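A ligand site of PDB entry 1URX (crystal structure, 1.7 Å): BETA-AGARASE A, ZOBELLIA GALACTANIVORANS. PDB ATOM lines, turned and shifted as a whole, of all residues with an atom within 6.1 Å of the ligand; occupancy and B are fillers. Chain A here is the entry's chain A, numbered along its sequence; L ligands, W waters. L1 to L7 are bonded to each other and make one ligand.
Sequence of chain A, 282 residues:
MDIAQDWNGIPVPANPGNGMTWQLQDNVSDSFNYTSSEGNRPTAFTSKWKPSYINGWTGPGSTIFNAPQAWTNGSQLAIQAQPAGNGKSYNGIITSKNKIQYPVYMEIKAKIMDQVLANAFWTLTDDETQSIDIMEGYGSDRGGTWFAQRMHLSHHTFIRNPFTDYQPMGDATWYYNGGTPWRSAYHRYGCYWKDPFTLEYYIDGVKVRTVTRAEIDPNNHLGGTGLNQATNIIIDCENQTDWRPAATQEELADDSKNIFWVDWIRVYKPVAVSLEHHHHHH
Water W15 lies within hydrogen-bond range of the side-chain amino group (NZ) of Lys 111 (2.7 Å) and an oxygen (O1) of LIG L1 (3.1 Å).
Water W3 bridges ND2 of Asn 73 and O4 of LG3 L3.
Water W14 bridges OH of Tyr 186 (3.2 Å) and O4 of LG2 L2 (3.3 Å).
Water W12 lies within hydrogen-bond range of the side-chain carboxylate of Asp 255 (2.5 Å) and an oxygen (O2) of LG3 L3 (3.5 Å).
Merely in contact with the ligand: Pro 68, Trp 71, Tyr 90, Tyr 186, Ile 259 and Trp 261.
Hydrophobic or aromatic side chains that line the ligand: Pro 68, Trp 71, Tyr 90, Ile 259 and Trp 261.
Of the 22 residues printed, 14 come within 4 Å of the ligand.
The nearest printed residue that does not touch the ligand is Pro 83 (4.1 Å).
An oxygen (O5) of LG6 L6 lies within hydrogen-bond range of the side-chain amide nitrogen of Gln 82.
O1 of LG4 L4 is in hydrogen-bond range of OD2 of Asp 255 (2.8 Å).
OE1 of Gln 69 sits close to O2 of LG5 L5 (2.9 Å).
ND2 of Asn 73 is in hydrogen-bond range of O5 of LG2 L2 (3.0 Å).
The side-chain amide nitrogen (ND2) of Asn 66 lies within hydrogen-bond range of an oxygen (O4) of LG7 L7 (3.0 Å).
An oxygen (O1) of LG4 L4 lies within hydrogen-bond range of the side-chain amide oxygen (OE1) of Gln 80 (3.1 Å).
NE2 of Gln 76 is in hydrogen-bond range of O5 of LG2 L2, at 3.2 Å.
An oxygen (O4) of LIG L1 sits at hydrogen-bond distance from the side-chain amino group of Lys 111 (3.4 Å).
The side-chain amide nitrogen (ND2) of Asn 258 sits at hydrogen-bond distance from the side-chain amide oxygen (OE1) of Gln 82.
O of Gln 69 is in hydrogen-bond range of N of Gln 80, 2.9 Å away.
The side-chain amide oxygen of Asn 73 lies within hydrogen-bond range of the backbone NH of Gln 76 (2.8 Å).
The backbone NH of Ser 75 is in hydrogen-bond range of the side-chain amide oxygen of Asn 73, 3.0 Å away.
The indole nitrogen of Trp 71 sits close to the side-chain amide nitrogen of Gln 80 (2.9 Å).
The side-chain amide oxygen of Gln 80 sits close to the side-chain amide oxygen of Asn 258.
OH of Tyr 186 lies within hydrogen-bond range of NE2 of Gln 76, at 2.5 Å.
The backbone carbonyl oxygen (O) of Trp 261 is in hydrogen-bond range of the backbone NH (N) of Lys 111, 2.9 Å away.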
ATOM      1  N   GLU A  38     -19.572  -9.280  22.725  1.00  0.00           N
ATOM      2  CA  GLU A  38     -20.263  -9.497  24.004  1.00  0.00           C
ATOM      3  C   GLU A  38     -19.651 -10.750  24.682  1.00  0.00           C
ATOM      4  O   GLU A  38     -19.462 -11.784  24.039  1.00  0.00           O
ATOM      5  CB  GLU A  38     -21.792  -9.629  23.777  1.00  0.00           C
ATOM      6  CG  GLU A  38     -22.647  -9.496  25.044  1.00  0.00           C
ATOM      7  CD  GLU A  38     -23.069  -8.052  25.382  1.00  0.00           C
ATOM      8  OE1 GLU A  38     -22.234  -7.102  25.299  1.00  0.00           O
ATOM      9  OE2 GLU A  38     -24.256  -7.845  25.760  1.00  0.00           O
ATOM     10  N   ASN A  66     -28.053  -1.460  21.067  1.00  0.00           N
ATOM     11  CA  ASN A  66     -27.907  -2.769  21.678  1.00  0.00           C
ATOM     12  C   ASN A  66     -26.455  -3.228  21.667  1.00  0.00           C
ATOM     13  O   ASN A  66     -25.810  -3.231  20.623  1.00  0.00           O
ATOM     14  CB  ASN A  66     -28.841  -3.764  20.952  1.00  0.00           C
ATOM     15  CG  ASN A  66     -29.111  -5.030  21.775  1.00  0.00           C
ATOM     16  OD1 ASN A  66     -29.312  -4.966  23.005  1.00  0.00           O
ATOM     17  ND2 ASN A  66     -29.083  -6.191  21.103  1.00  0.00           N
ATOM     18  N   PRO A  68     -24.567  -6.004  21.961  1.00  0.00           N
ATOM     19  CA  PRO A  68     -24.017  -7.094  21.130  1.00  0.00           C
ATOM     20  C   PRO A  68     -23.714  -6.713  19.695  1.00  0.00           C
ATOM     21  O   PRO A  68     -22.910  -7.354  19.067  1.00  0.00           O
ATOM     22  CB  PRO A  68     -25.100  -8.175  21.178  1.00  0.00           C
ATOM     23  CG  PRO A  68     -25.943  -7.840  22.342  1.00  0.00           C
ATOM     24  CD  PRO A  68     -25.857  -6.353  22.583  1.00  0.00           C
ATOM     25  N   GLN A  69     -24.356  -5.662  19.167  1.00  0.00           N
ATOM     26  CA  GLN A  69     -24.157  -5.325  17.781  1.00  0.00           C
ATOM     27  C   GLN A  69     -22.927  -4.431  17.526  1.00  0.00           C
ATOM     28  O   GLN A  69     -22.707  -3.983  16.397  1.00  0.00           O
ATOM     29  CB  GLN A  69     -25.441  -4.717  17.217  1.00  0.00           C
ATOM     30  CG  GLN A  69     -26.417  -5.778  16.687  1.00  0.00           C
ATOM     31  CD  GLN A  69     -27.167  -6.473  17.773  1.00  0.00           C
ATOM     32  OE1 GLN A  69     -27.332  -7.742  17.763  1.00  0.00           O
ATOM     33  NE2 GLN A  69     -27.673  -5.729  18.675  1.00  0.00           N
ATOM     34  N   ALA A  70     -22.114  -4.190  18.553  1.00  0.00           N
ATOM     35  CA  ALA A  70     -20.777  -3.658  18.346  1.00  0.00           C
ATOM     36  C   ALA A  70     -19.775  -4.767  18.664  1.00  0.00           C
ATOM     37  O   ALA A  70     -19.833  -5.312  19.732  1.00  0.00           O
ATOM     38  CB  ALA A  70     -20.511  -2.465  19.204  1.00  0.00           C
ATOM     39  N   TRP A  71     -18.874  -5.034  17.745  1.00  0.00           N
ATOM     40  CA  TRP A  71     -17.827  -6.072  17.913  1.00  0.00           C
ATOM     41  C   TRP A  71     -16.667  -5.869  16.965  1.00  0.00           C
ATOM     42  O   TRP A  71     -16.763  -5.068  16.079  1.00  0.00           O
ATOM     43  CB  TRP A  71     -18.443  -7.478  17.811  1.00  0.00           C
ATOM     44  CG  TRP A  71     -19.255  -7.716  16.581  1.00  0.00           C
ATOM     45  CD1 TRP A  71     -20.579  -7.417  16.400  1.00  0.00           C
ATOM     46  CD2 TRP A  71     -18.815  -8.299  15.347  1.00  0.00           C
ATOM     47  NE1 TRP A  71     -20.989  -7.770  15.138  1.00  0.00           N
ATOM     48  CE2 TRP A  71     -19.930  -8.317  14.468  1.00  0.00           C
ATOM     49  CE3 TRP A  71     -17.600  -8.806  14.895  1.00  0.00           C
ATOM     50  CZ2 TRP A  71     -19.856  -8.804  13.165  1.00  0.00           C
ATOM     51  CZ3 TRP A  71     -17.522  -9.294  13.579  1.00  0.00           C
ATOM     52  CH2 TRP A  71     -18.642  -9.278  12.741  1.00  0.00           C
ATOM     53  N   THR A  72     -15.527  -6.568  17.161  1.00  0.00           N
ATOM     54  CA  THR A  72     -14.395  -6.483  16.246  1.00  0.00           C
ATOM     55  C   THR A  72     -13.907  -7.854  15.828  1.00  0.00           C
ATOM     56  O   THR A  72     -14.088  -8.813  16.571  1.00  0.00           O
ATOM     57  CB  THR A  72     -13.227  -5.736  16.882  1.00  0.00           C
ATOM     58  OG1 THR A  72     -12.764  -6.461  18.007  1.00  0.00           O
ATOM     59  CG2 THR A  72     -13.686  -4.382  17.489  1.00  0.00           C
ATOM     60  N   ASN A  73     -13.299  -7.931  14.645  1.00  0.00           N
ATOM     61  CA  ASN A  73     -13.022  -9.243  13.993  1.00  0.00           C
ATOM     62  C   ASN A  73     -11.538  -9.523  13.790  1.00  0.00           C
ATOM     63  O   ASN A  73     -11.172 -10.389  12.989  1.00  0.00           O
ATOM     64  CB  ASN A  73     -13.763  -9.339  12.638  1.00  0.00           C
ATOM     65  CG  ASN A  73     -13.167  -8.421  11.589  1.00  0.00           C
ATOM     66  OD1 ASN A  73     -12.216  -7.688  11.882  1.00  0.00           O
ATOM     67  ND2 ASN A  73     -13.731  -8.427  10.369  1.00  0.00           N
ATOM     68  N   SER A  75      -9.389  -7.182  12.711  1.00  0.00           N
ATOM     69  CA  SER A  75      -8.870  -6.109  11.895  1.00  0.00           C
ATOM     70  C   SER A  75      -9.815  -4.879  11.835  1.00  0.00           C
ATOM     71  O   SER A  75      -9.334  -3.786  11.605  1.00  0.00           O
ATOM     72  CB  SER A  75      -8.535  -6.569  10.480  1.00  0.00           C
ATOM     73  OG  SER A  75      -9.667  -7.062   9.797  1.00  0.00           O
ATOM     74  N   GLN A  76     -11.121  -5.073  12.012  1.00  0.00           N
ATOM     75  CA  GLN A  76     -12.102  -3.984  11.888  1.00  0.00           C
ATOM     76  C   GLN A  76     -13.172  -4.027  12.970  1.00  0.00           C
ATOM     77  O   GLN A  76     -13.516  -5.098  13.516  1.00  0.00           O
ATOM     78  CB  GLN A  76     -12.742  -4.044  10.513  1.00  0.00           C
ATOM     79  CG  GLN A  76     -11.717  -4.014   9.414  1.00  0.00           C
ATOM     80  CD  GLN A  76     -12.254  -3.817   8.057  1.00  0.00           C
ATOM     81  OE1 GLN A  76     -11.495  -3.930   7.079  1.00  0.00           O
ATOM     82  NE2 GLN A  76     -13.552  -3.609   7.943  1.00  0.00           N
ATOM     83  N   GLN A  80     -23.133  -3.225  13.629  1.00  0.00           N
ATOM     84  CA  GLN A  80     -24.085  -4.076  12.939  1.00  0.00           C
ATOM     85  C   GLN A  80     -25.510  -3.739  13.271  1.00  0.00           C
ATOM     86  O   GLN A  80     -25.821  -3.228  14.363  1.00  0.00           O
ATOM     87  CB  GLN A  80     -23.799  -5.561  13.260  1.00  0.00           C
ATOM     88  CG  GLN A  80     -24.552  -6.584  12.375  1.00  0.00           C
ATOM     89  CD  GLN A  80     -23.978  -8.003  12.452  1.00  0.00           C
ATOM     90  OE1 GLN A  80     -24.150  -8.816  11.505  1.00  0.00           O
ATOM     91  NE2 GLN A  80     -23.321  -8.298  13.512  1.00  0.00           N
ATOM     92  N   ALA A  81     -26.398  -4.055  12.330  1.00  0.00           N
ATOM     93  CA  ALA A  81     -27.838  -3.997  12.585  1.00  0.00           C
ATOM     94  C   ALA A  81     -28.421  -5.408  12.572  1.00  0.00           C
ATOM     95  O   ALA A  81     -27.879  -6.295  11.945  1.00  0.00           O
ATOM     96  CB  ALA A  81     -28.552  -3.140  11.600  1.00  0.00           C
ATOM     97  N   GLN A  82     -29.517  -5.581  13.309  1.00  0.00           N
ATOM     98  CA  GLN A  82     -30.242  -6.861  13.324  1.00  0.00           C
ATOM     99  C   GLN A  82     -31.742  -6.621  13.357  1.00  0.00           C
ATOM    100  O   GLN A  82     -32.231  -5.543  13.752  1.00  0.00           O
ATOM    101  CB  GLN A  82     -29.867  -7.695  14.539  1.00  0.00           C
ATOM    102  CG  GLN A  82     -28.543  -8.312  14.524  1.00  0.00           C
ATOM    103  CD  GLN A  82     -28.449  -9.426  13.481  1.00  0.00           C
ATOM    104  OE1 GLN A  82     -27.927  -9.229  12.365  1.00  0.00           O
ATOM    105  NE2 GLN A  82     -28.909 -10.584  13.855  1.00  0.00           N
ATOM    106  N   PRO A  83     -32.509  -7.626  12.962  1.00  0.00           N
ATOM    107  CA  PRO A  83     -33.964  -7.542  13.090  1.00  0.00           C
ATOM    108  C   PRO A  83     -34.358  -7.510  14.537  1.00  0.00           C
ATOM    109  O   PRO A  83     -33.832  -8.301  15.308  1.00  0.00           O
ATOM    110  CB  PRO A  83     -34.456  -8.869  12.457  1.00  0.00           C
ATOM    111  CG  PRO A  83     -33.345  -9.347  11.702  1.00  0.00           C
ATOM    112  CD  PRO A  83     -32.086  -8.913  12.396  1.00  0.00           C
ATOM    113  N   TYR A  90     -32.289  -3.745  15.996  1.00  0.00           N
ATOM    114  CA  TYR A  90     -31.257  -3.602  17.012  1.00  0.00           C
ATOM    115  C   TYR A  90     -30.071  -2.958  16.286  1.00  0.00           C
ATOM    116  O   TYR A  90     -29.783  -3.292  15.141  1.00  0.00           O
ATOM    117  CB  TYR A  90     -30.841  -4.943  17.638  1.00  0.00           C
ATOM    118  CG  TYR A  90     -31.939  -5.567  18.450  1.00  0.00           C
ATOM    119  CD1 TYR A  90     -32.409  -6.827  18.155  1.00  0.00           C
ATOM    120  CD2 TYR A  90     -32.538  -4.865  19.512  1.00  0.00           C
ATOM    121  CE1 TYR A  90     -33.467  -7.386  18.881  1.00  0.00           C
ATOM    122  CE2 TYR A  90     -33.581  -5.430  20.241  1.00  0.00           C
ATOM    123  CZ  TYR A  90     -34.026  -6.706  19.924  1.00  0.00           C
ATOM    124  OH  TYR A  90     -35.064  -7.269  20.662  1.00  0.00           O
ATOM    125  N   LYS A 111     -16.569   1.768   5.644  1.00  0.00           N
ATOM    126  CA  LYS A 111     -17.435   1.400   4.512  1.00  0.00           C
ATOM    127  C   LYS A 111     -18.875   1.281   5.012  1.00  0.00           C
ATOM    128  O   LYS A 111     -19.182   0.401   5.846  1.00  0.00           O
ATOM    129  CB  LYS A 111     -16.976   0.068   3.912  1.00  0.00           C
ATOM    130  CG  LYS A 111     -17.751  -0.403   2.645  1.00  0.00           C
ATOM    131  CD  LYS A 111     -17.060  -1.628   2.083  1.00  0.00           C
ATOM    132  CE  LYS A 111     -17.789  -2.321   0.985  1.00  0.00           C
ATOM    133  NZ  LYS A 111     -16.878  -3.477   0.562  1.00  0.00           N
ATOM    134  N   TYR A 186     -14.392   1.389   0.997  1.00  0.00           N
ATOM    135  CA  TYR A 186     -13.871   2.123   2.124  1.00  0.00           C
ATOM    136  C   TYR A 186     -13.418   3.510   1.663  1.00  0.00           C
ATOM    137  O   TYR A 186     -12.802   3.683   0.592  1.00  0.00           O
ATOM    138  CB  TYR A 186     -12.709   1.411   2.821  1.00  0.00           C
ATOM    139  CG  TYR A 186     -13.104   0.158   3.584  1.00  0.00           C
ATOM    140  CD1 TYR A 186     -13.334  -1.039   2.931  1.00  0.00           C
ATOM    141  CD2 TYR A 186     -13.272   0.171   4.962  1.00  0.00           C
ATOM    142  CE1 TYR A 186     -13.674  -2.159   3.617  1.00  0.00           C
ATOM    143  CE2 TYR A 186     -13.640  -0.966   5.657  1.00  0.00           C
ATOM    144  CZ  TYR A 186     -13.838  -2.137   4.967  1.00  0.00           C
ATOM    145  OH  TYR A 186     -14.259  -3.303   5.605  1.00  0.00           O
ATOM    146  N   ASP A 255     -26.459 -10.600   6.705  1.00  0.00           N
ATOM    147  CA  ASP A 255     -25.146 -10.168   7.201  1.00  0.00           C
ATOM    148  C   ASP A 255     -24.056  -9.878   6.154  1.00  0.00           C
ATOM    149  O   ASP A 255     -22.957  -9.434   6.489  1.00  0.00           O
ATOM    150  CB  ASP A 255     -24.671 -10.931   8.446  1.00  0.00           C
ATOM    151  CG  ASP A 255     -24.352 -12.353   8.199  1.00  0.00           C
ATOM    152  OD1 ASP A 255     -24.851 -12.894   7.189  1.00  0.00           O
ATOM    153  OD2 ASP A 255     -23.661 -13.023   9.021  1.00  0.00           O
ATOM    154  N   SER A 256     -24.400 -10.037   4.889  1.00  0.00           N
ATOM    155  CA  SER A 256     -23.564  -9.525   3.820  1.00  0.00           C
ATOM    156  C   SER A 256     -23.766  -8.033   3.577  1.00  0.00           C
ATOM    157  O   SER A 256     -23.023  -7.415   2.810  1.00  0.00           O
ATOM    158  CB  SER A 256     -23.824 -10.320   2.517  1.00  0.00           C
ATOM    159  OG  SER A 256     -24.972  -9.842   1.822  1.00  0.00           O
ATOM    160  N   ASN A 258     -25.442  -5.861   6.425  1.00  0.00           N
ATOM    161  CA  ASN A 258     -25.934  -5.190   7.644  1.00  0.00           C
ATOM    162  C   ASN A 258     -24.823  -4.732   8.585  1.00  0.00           C
ATOM    163  O   ASN A 258     -25.094  -4.453   9.758  1.00  0.00           O
ATOM    164  CB  ASN A 258     -26.959  -6.040   8.385  1.00  0.00           C
ATOM    165  CG  ASN A 258     -26.363  -7.319   8.936  1.00  0.00           C
ATOM    166  OD1 ASN A 258     -25.152  -7.488   8.927  1.00  0.00           O
ATOM    167  ND2 ASN A 258     -27.210  -8.237   9.423  1.00  0.00           N
ATOM    168  N   ILE A 259     -23.591  -4.608   8.065  1.00  0.00           N
ATOM    169  CA  ILE A 259     -22.447  -4.162   8.883  1.00  0.00           C
ATOM    170  C   ILE A 259     -21.800  -2.901   8.289  1.00  0.00           C
ATOM    171  O   ILE A 259     -21.442  -2.825   7.122  1.00  0.00           O
ATOM    172  CB  ILE A 259     -21.357  -5.269   9.077  1.00  0.00           C
ATOM    173  CG1 ILE A 259     -21.967  -6.492   9.758  1.00  0.00           C
ATOM    174  CG2 ILE A 259     -20.194  -4.723   9.919  1.00  0.00           C
ATOM    175  CD1 ILE A 259     -21.132  -7.695   9.616  1.00  0.00           C
ATOM    176  N   TRP A 261     -18.551  -1.089   8.528  1.00  0.00           N
ATOM    177  CA  TRP A 261     -17.176  -1.528   8.855  1.00  0.00           C
ATOM    178  C   TRP A 261     -16.280  -0.309   9.050  1.00  0.00           C
ATOM    179  O   TRP A 261     -16.240   0.562   8.210  1.00  0.00           O
ATOM    180  CB  TRP A 261     -16.573  -2.410   7.740  1.00  0.00           C
ATOM    181  CG  TRP A 261     -17.160  -3.788   7.638  1.00  0.00           C
ATOM    182  CD1 TRP A 261     -17.980  -4.277   6.652  1.00  0.00           C
ATOM    183  CD2 TRP A 261     -16.948  -4.857   8.544  1.00  0.00           C
ATOM    184  NE1 TRP A 261     -18.310  -5.587   6.915  1.00  0.00           N
ATOM    185  CE2 TRP A 261     -17.683  -5.964   8.072  1.00  0.00           C
ATOM    186  CE3 TRP A 261     -16.242  -4.983   9.735  1.00  0.00           C
ATOM    187  CZ2 TRP A 261     -17.700  -7.186   8.758  1.00  0.00           C
ATOM    188  CZ3 TRP A 261     -16.239  -6.201  10.397  1.00  0.00           C
ATOM    189  CH2 TRP A 261     -16.979  -7.280   9.909  1.00  0.00           C
HETATM  190  C1  LIG L   1     -16.661  -6.566  -0.893  1.00  0.00           C
HETATM  191  C2  LIG L   1     -15.200  -7.053  -0.784  1.00  0.00           C
HETATM  192  C3  LIG L   1     -15.045  -8.258   0.176  1.00  0.00           C
HETATM  193  C4  LIG L   1     -15.841  -8.214   1.431  1.00  0.00           C
HETATM  194  C5  LIG L   1     -17.217  -8.052   0.899  1.00  0.00           C
HETATM  195  C6  LIG L   1     -17.166  -9.252  -0.050  1.00  0.00           C
HETATM  196  O1  LIG L   1     -14.344  -5.994  -0.384  1.00  0.00           O
HETATM  197  O2  LIG L   1     -15.757  -9.367  -0.392  1.00  0.00           O
HETATM  198  O3  LIG L   1     -15.942  -9.008   2.633  1.00  0.00           O
HETATM  199  O4  LIG L   1     -17.477  -6.796   0.262  1.00  0.00           O
HETATM  200  C1  LG2 L   2     -15.766  -8.673   3.919  1.00  0.00           C
HETATM  201  C2  LG2 L   2     -16.125  -9.957   4.692  1.00  0.00           C
HETATM  202  C3  LG2 L   2     -16.315  -9.679   6.196  1.00  0.00           C
HETATM  203  C4  LG2 L   2     -15.182  -8.839   6.806  1.00  0.00           C
HETATM  204  C5  LG2 L   2     -14.911  -7.597   5.941  1.00  0.00           C
HETATM  205  C6  LG2 L   2     -13.719  -6.779   6.485  1.00  0.00           C
HETATM  206  O1  LG2 L   2     -17.315 -10.482   4.170  1.00  0.00           O
HETATM  207  O2  LG2 L   2     -16.449 -10.908   6.906  1.00  0.00           O
HETATM  208  O3  LG2 L   2     -14.001  -9.599   6.898  1.00  0.00           O
HETATM  209  O4  LG2 L   2     -14.729  -7.940   4.552  1.00  0.00           O
HETATM  210  O5  LG2 L   2     -13.547  -6.786   7.916  1.00  0.00           O
HETATM  211  C1  LG3 L   3     -17.761 -11.271   7.318  1.00  0.00           C
HETATM  212  C2  LG3 L   3     -17.676 -12.730   7.823  1.00  0.00           C
HETATM  213  C3  LG3 L   3     -19.042 -13.202   8.342  1.00  0.00           C
HETATM  214  C4  LG3 L   3     -19.420 -12.439   9.543  1.00  0.00           C
HETATM  215  C5  LG3 L   3     -19.544 -11.046   8.993  1.00  0.00           C
HETATM  216  C6  LG3 L   3     -20.537 -11.414   7.889  1.00  0.00           C
HETATM  217  O1  LG3 L   3     -16.507 -13.152   8.493  1.00  0.00           O
HETATM  218  O2  LG3 L   3     -20.121 -12.758   7.519  1.00  0.00           O
HETATM  219  O3  LG3 L   3     -20.425 -12.757  10.486  1.00  0.00           O
HETATM  220  O4  LG3 L   3     -18.325 -10.524   8.431  1.00  0.00           O
HETATM  221  C1  LG4 L   4     -20.544 -12.258  11.705  1.00  0.00           C
HETATM  222  C2  LG4 L   4     -22.001 -12.399  12.114  1.00  0.00           C
HETATM  223  C3  LG4 L   4     -22.186 -12.009  13.588  1.00  0.00           C
HETATM  224  C4  LG4 L   4     -21.156 -12.793  14.451  1.00  0.00           C
HETATM  225  C5  LG4 L   4     -19.739 -12.687  13.873  1.00  0.00           C
HETATM  226  C6  LG4 L   4     -18.819 -13.632  14.662  1.00  0.00           C
HETATM  227  O1  LG4 L   4     -22.823 -11.632  11.250  1.00  0.00           O
HETATM  228  O2  LG4 L   4     -23.534 -12.310  13.852  1.00  0.00           O
HETATM  229  O3  LG4 L   4     -21.491 -14.173  14.402  1.00  0.00           O
HETATM  230  O4  LG4 L   4     -19.681 -13.051  12.491  1.00  0.00           O
HETATM  231  O5  LG4 L   4     -17.470 -13.328  14.420  1.00  0.00           O
HETATM  232  C1  LG5 L   5     -24.070 -11.349  14.719  1.00  0.00           C
HETATM  233  C2  LG5 L   5     -25.582 -11.545  14.781  1.00  0.00           C
HETATM  234  C3  LG5 L   5     -26.245 -10.744  15.869  1.00  0.00           C
HETATM  235  C4  LG5 L   5     -25.787 -11.193  17.190  1.00  0.00           C
HETATM  236  C5  LG5 L   5     -24.327 -10.920  17.092  1.00  0.00           C
HETATM  237  C6  LG5 L   5     -24.515  -9.412  16.742  1.00  0.00           C
HETATM  238  O1  LG5 L   5     -26.153 -12.854  14.594  1.00  0.00           O
HETATM  239  O2  LG5 L   5     -25.725  -9.406  15.948  1.00  0.00           O
HETATM  240  O3  LG5 L   5     -26.238 -10.867  18.492  1.00  0.00           O
HETATM  241  O4  LG5 L   5     -23.611 -11.609  16.065  1.00  0.00           O
HETATM  242  C1  LG6 L   6     -27.510 -11.165  18.687  1.00  0.00           C
HETATM  243  C2  LG6 L   6     -27.700 -10.644  20.121  1.00  0.00           C
HETATM  244  C3  LG6 L   6     -29.157 -10.627  20.562  1.00  0.00           C
HETATM  245  C4  LG6 L   6     -30.126 -10.080  19.530  1.00  0.00           C
HETATM  246  C5  LG6 L   6     -29.828 -10.832  18.208  1.00  0.00           C
HETATM  247  C6  LG6 L   6     -30.725 -10.381  17.050  1.00  0.00           C
HETATM  248  O1  LG6 L   6     -26.918 -11.396  21.040  1.00  0.00           O
HETATM  249  O2  LG6 L   6     -29.165  -9.920  21.795  1.00  0.00           O
HETATM  250  O3  LG6 L   6     -29.854  -8.702  19.273  1.00  0.00           O
HETATM  251  O4  LG6 L   6     -28.473 -10.643  17.825  1.00  0.00           O
HETATM  252  O5  LG6 L   6     -30.563 -11.245  15.931  1.00  0.00           O
HETATM  253  C1  LG7 L   7     -30.448  -9.592  22.308  1.00  0.00           C
HETATM  254  C2  LG7 L   7     -30.221  -9.430  23.843  1.00  0.00           C
HETATM  255  C3  LG7 L   7     -31.495  -8.976  24.580  1.00  0.00           C
HETATM  256  C4  LG7 L   7     -31.891  -7.616  24.104  1.00  0.00           C
HETATM  257  C5  LG7 L   7     -32.193  -7.914  22.671  1.00  0.00           C
HETATM  258  C6  LG7 L   7     -33.249  -8.996  22.987  1.00  0.00           C
HETATM  259  O1  LG7 L   7     -28.955  -9.024  24.313  1.00  0.00           O
HETATM  260  O2  LG7 L   7     -32.702  -9.674  24.146  1.00  0.00           O
HETATM  261  O3  LG7 L   7     -32.822  -6.636  24.606  1.00  0.00           O
HETATM  262  O4  LG7 L   7     -31.069  -8.372  21.868  1.00  0.00           O
HETATM  263  O   HOH W   1     -20.476 -10.700  17.243  1.00  0.00           O
HETATM  264  O   HOH W   2     -32.656 -12.533  14.394  1.00  0.00           O
HETATM  265  O   HOH W   3     -15.824 -10.548  10.234  1.00  0.00           O
HETATM  266  O   HOH W   4     -16.597 -15.909  14.436  1.00  0.00           O
HETATM  267  O   HOH W   5     -18.216 -11.919  16.892  1.00  0.00           O
HETATM  268  O   HOH W   6     -15.928 -12.399  12.180  1.00  0.00           O
HETATM  269  O   HOH W   7     -28.622 -13.984  16.018  1.00  0.00           O
HETATM  270  O   HOH W   8     -24.251 -11.994  20.867  1.00  0.00           O
HETATM  271  O   HOH W   9     -24.101 -14.732  15.416  1.00  0.00           O
HETATM  272  O   HOH W  10     -14.981 -12.132  14.890  1.00  0.00           O
HETATM  273  O   HOH W  11     -27.068 -10.838  23.864  1.00  0.00           O
HETATM  274  O   HOH W  12     -22.411 -15.161   8.565  1.00  0.00           O
HETATM  275  O   HOH W  13     -25.988 -13.003  11.661  1.00  0.00           O
HETATM  276  O   HOH W  14     -16.138  -5.080   3.753  1.00  0.00           O
HETATM  277  O   HOH W  15     -14.327  -2.938  -0.269  1.00  0.00           O
HETATM  278  O   HOH W  16     -30.970  -6.281  27.365  1.00  0.00           O
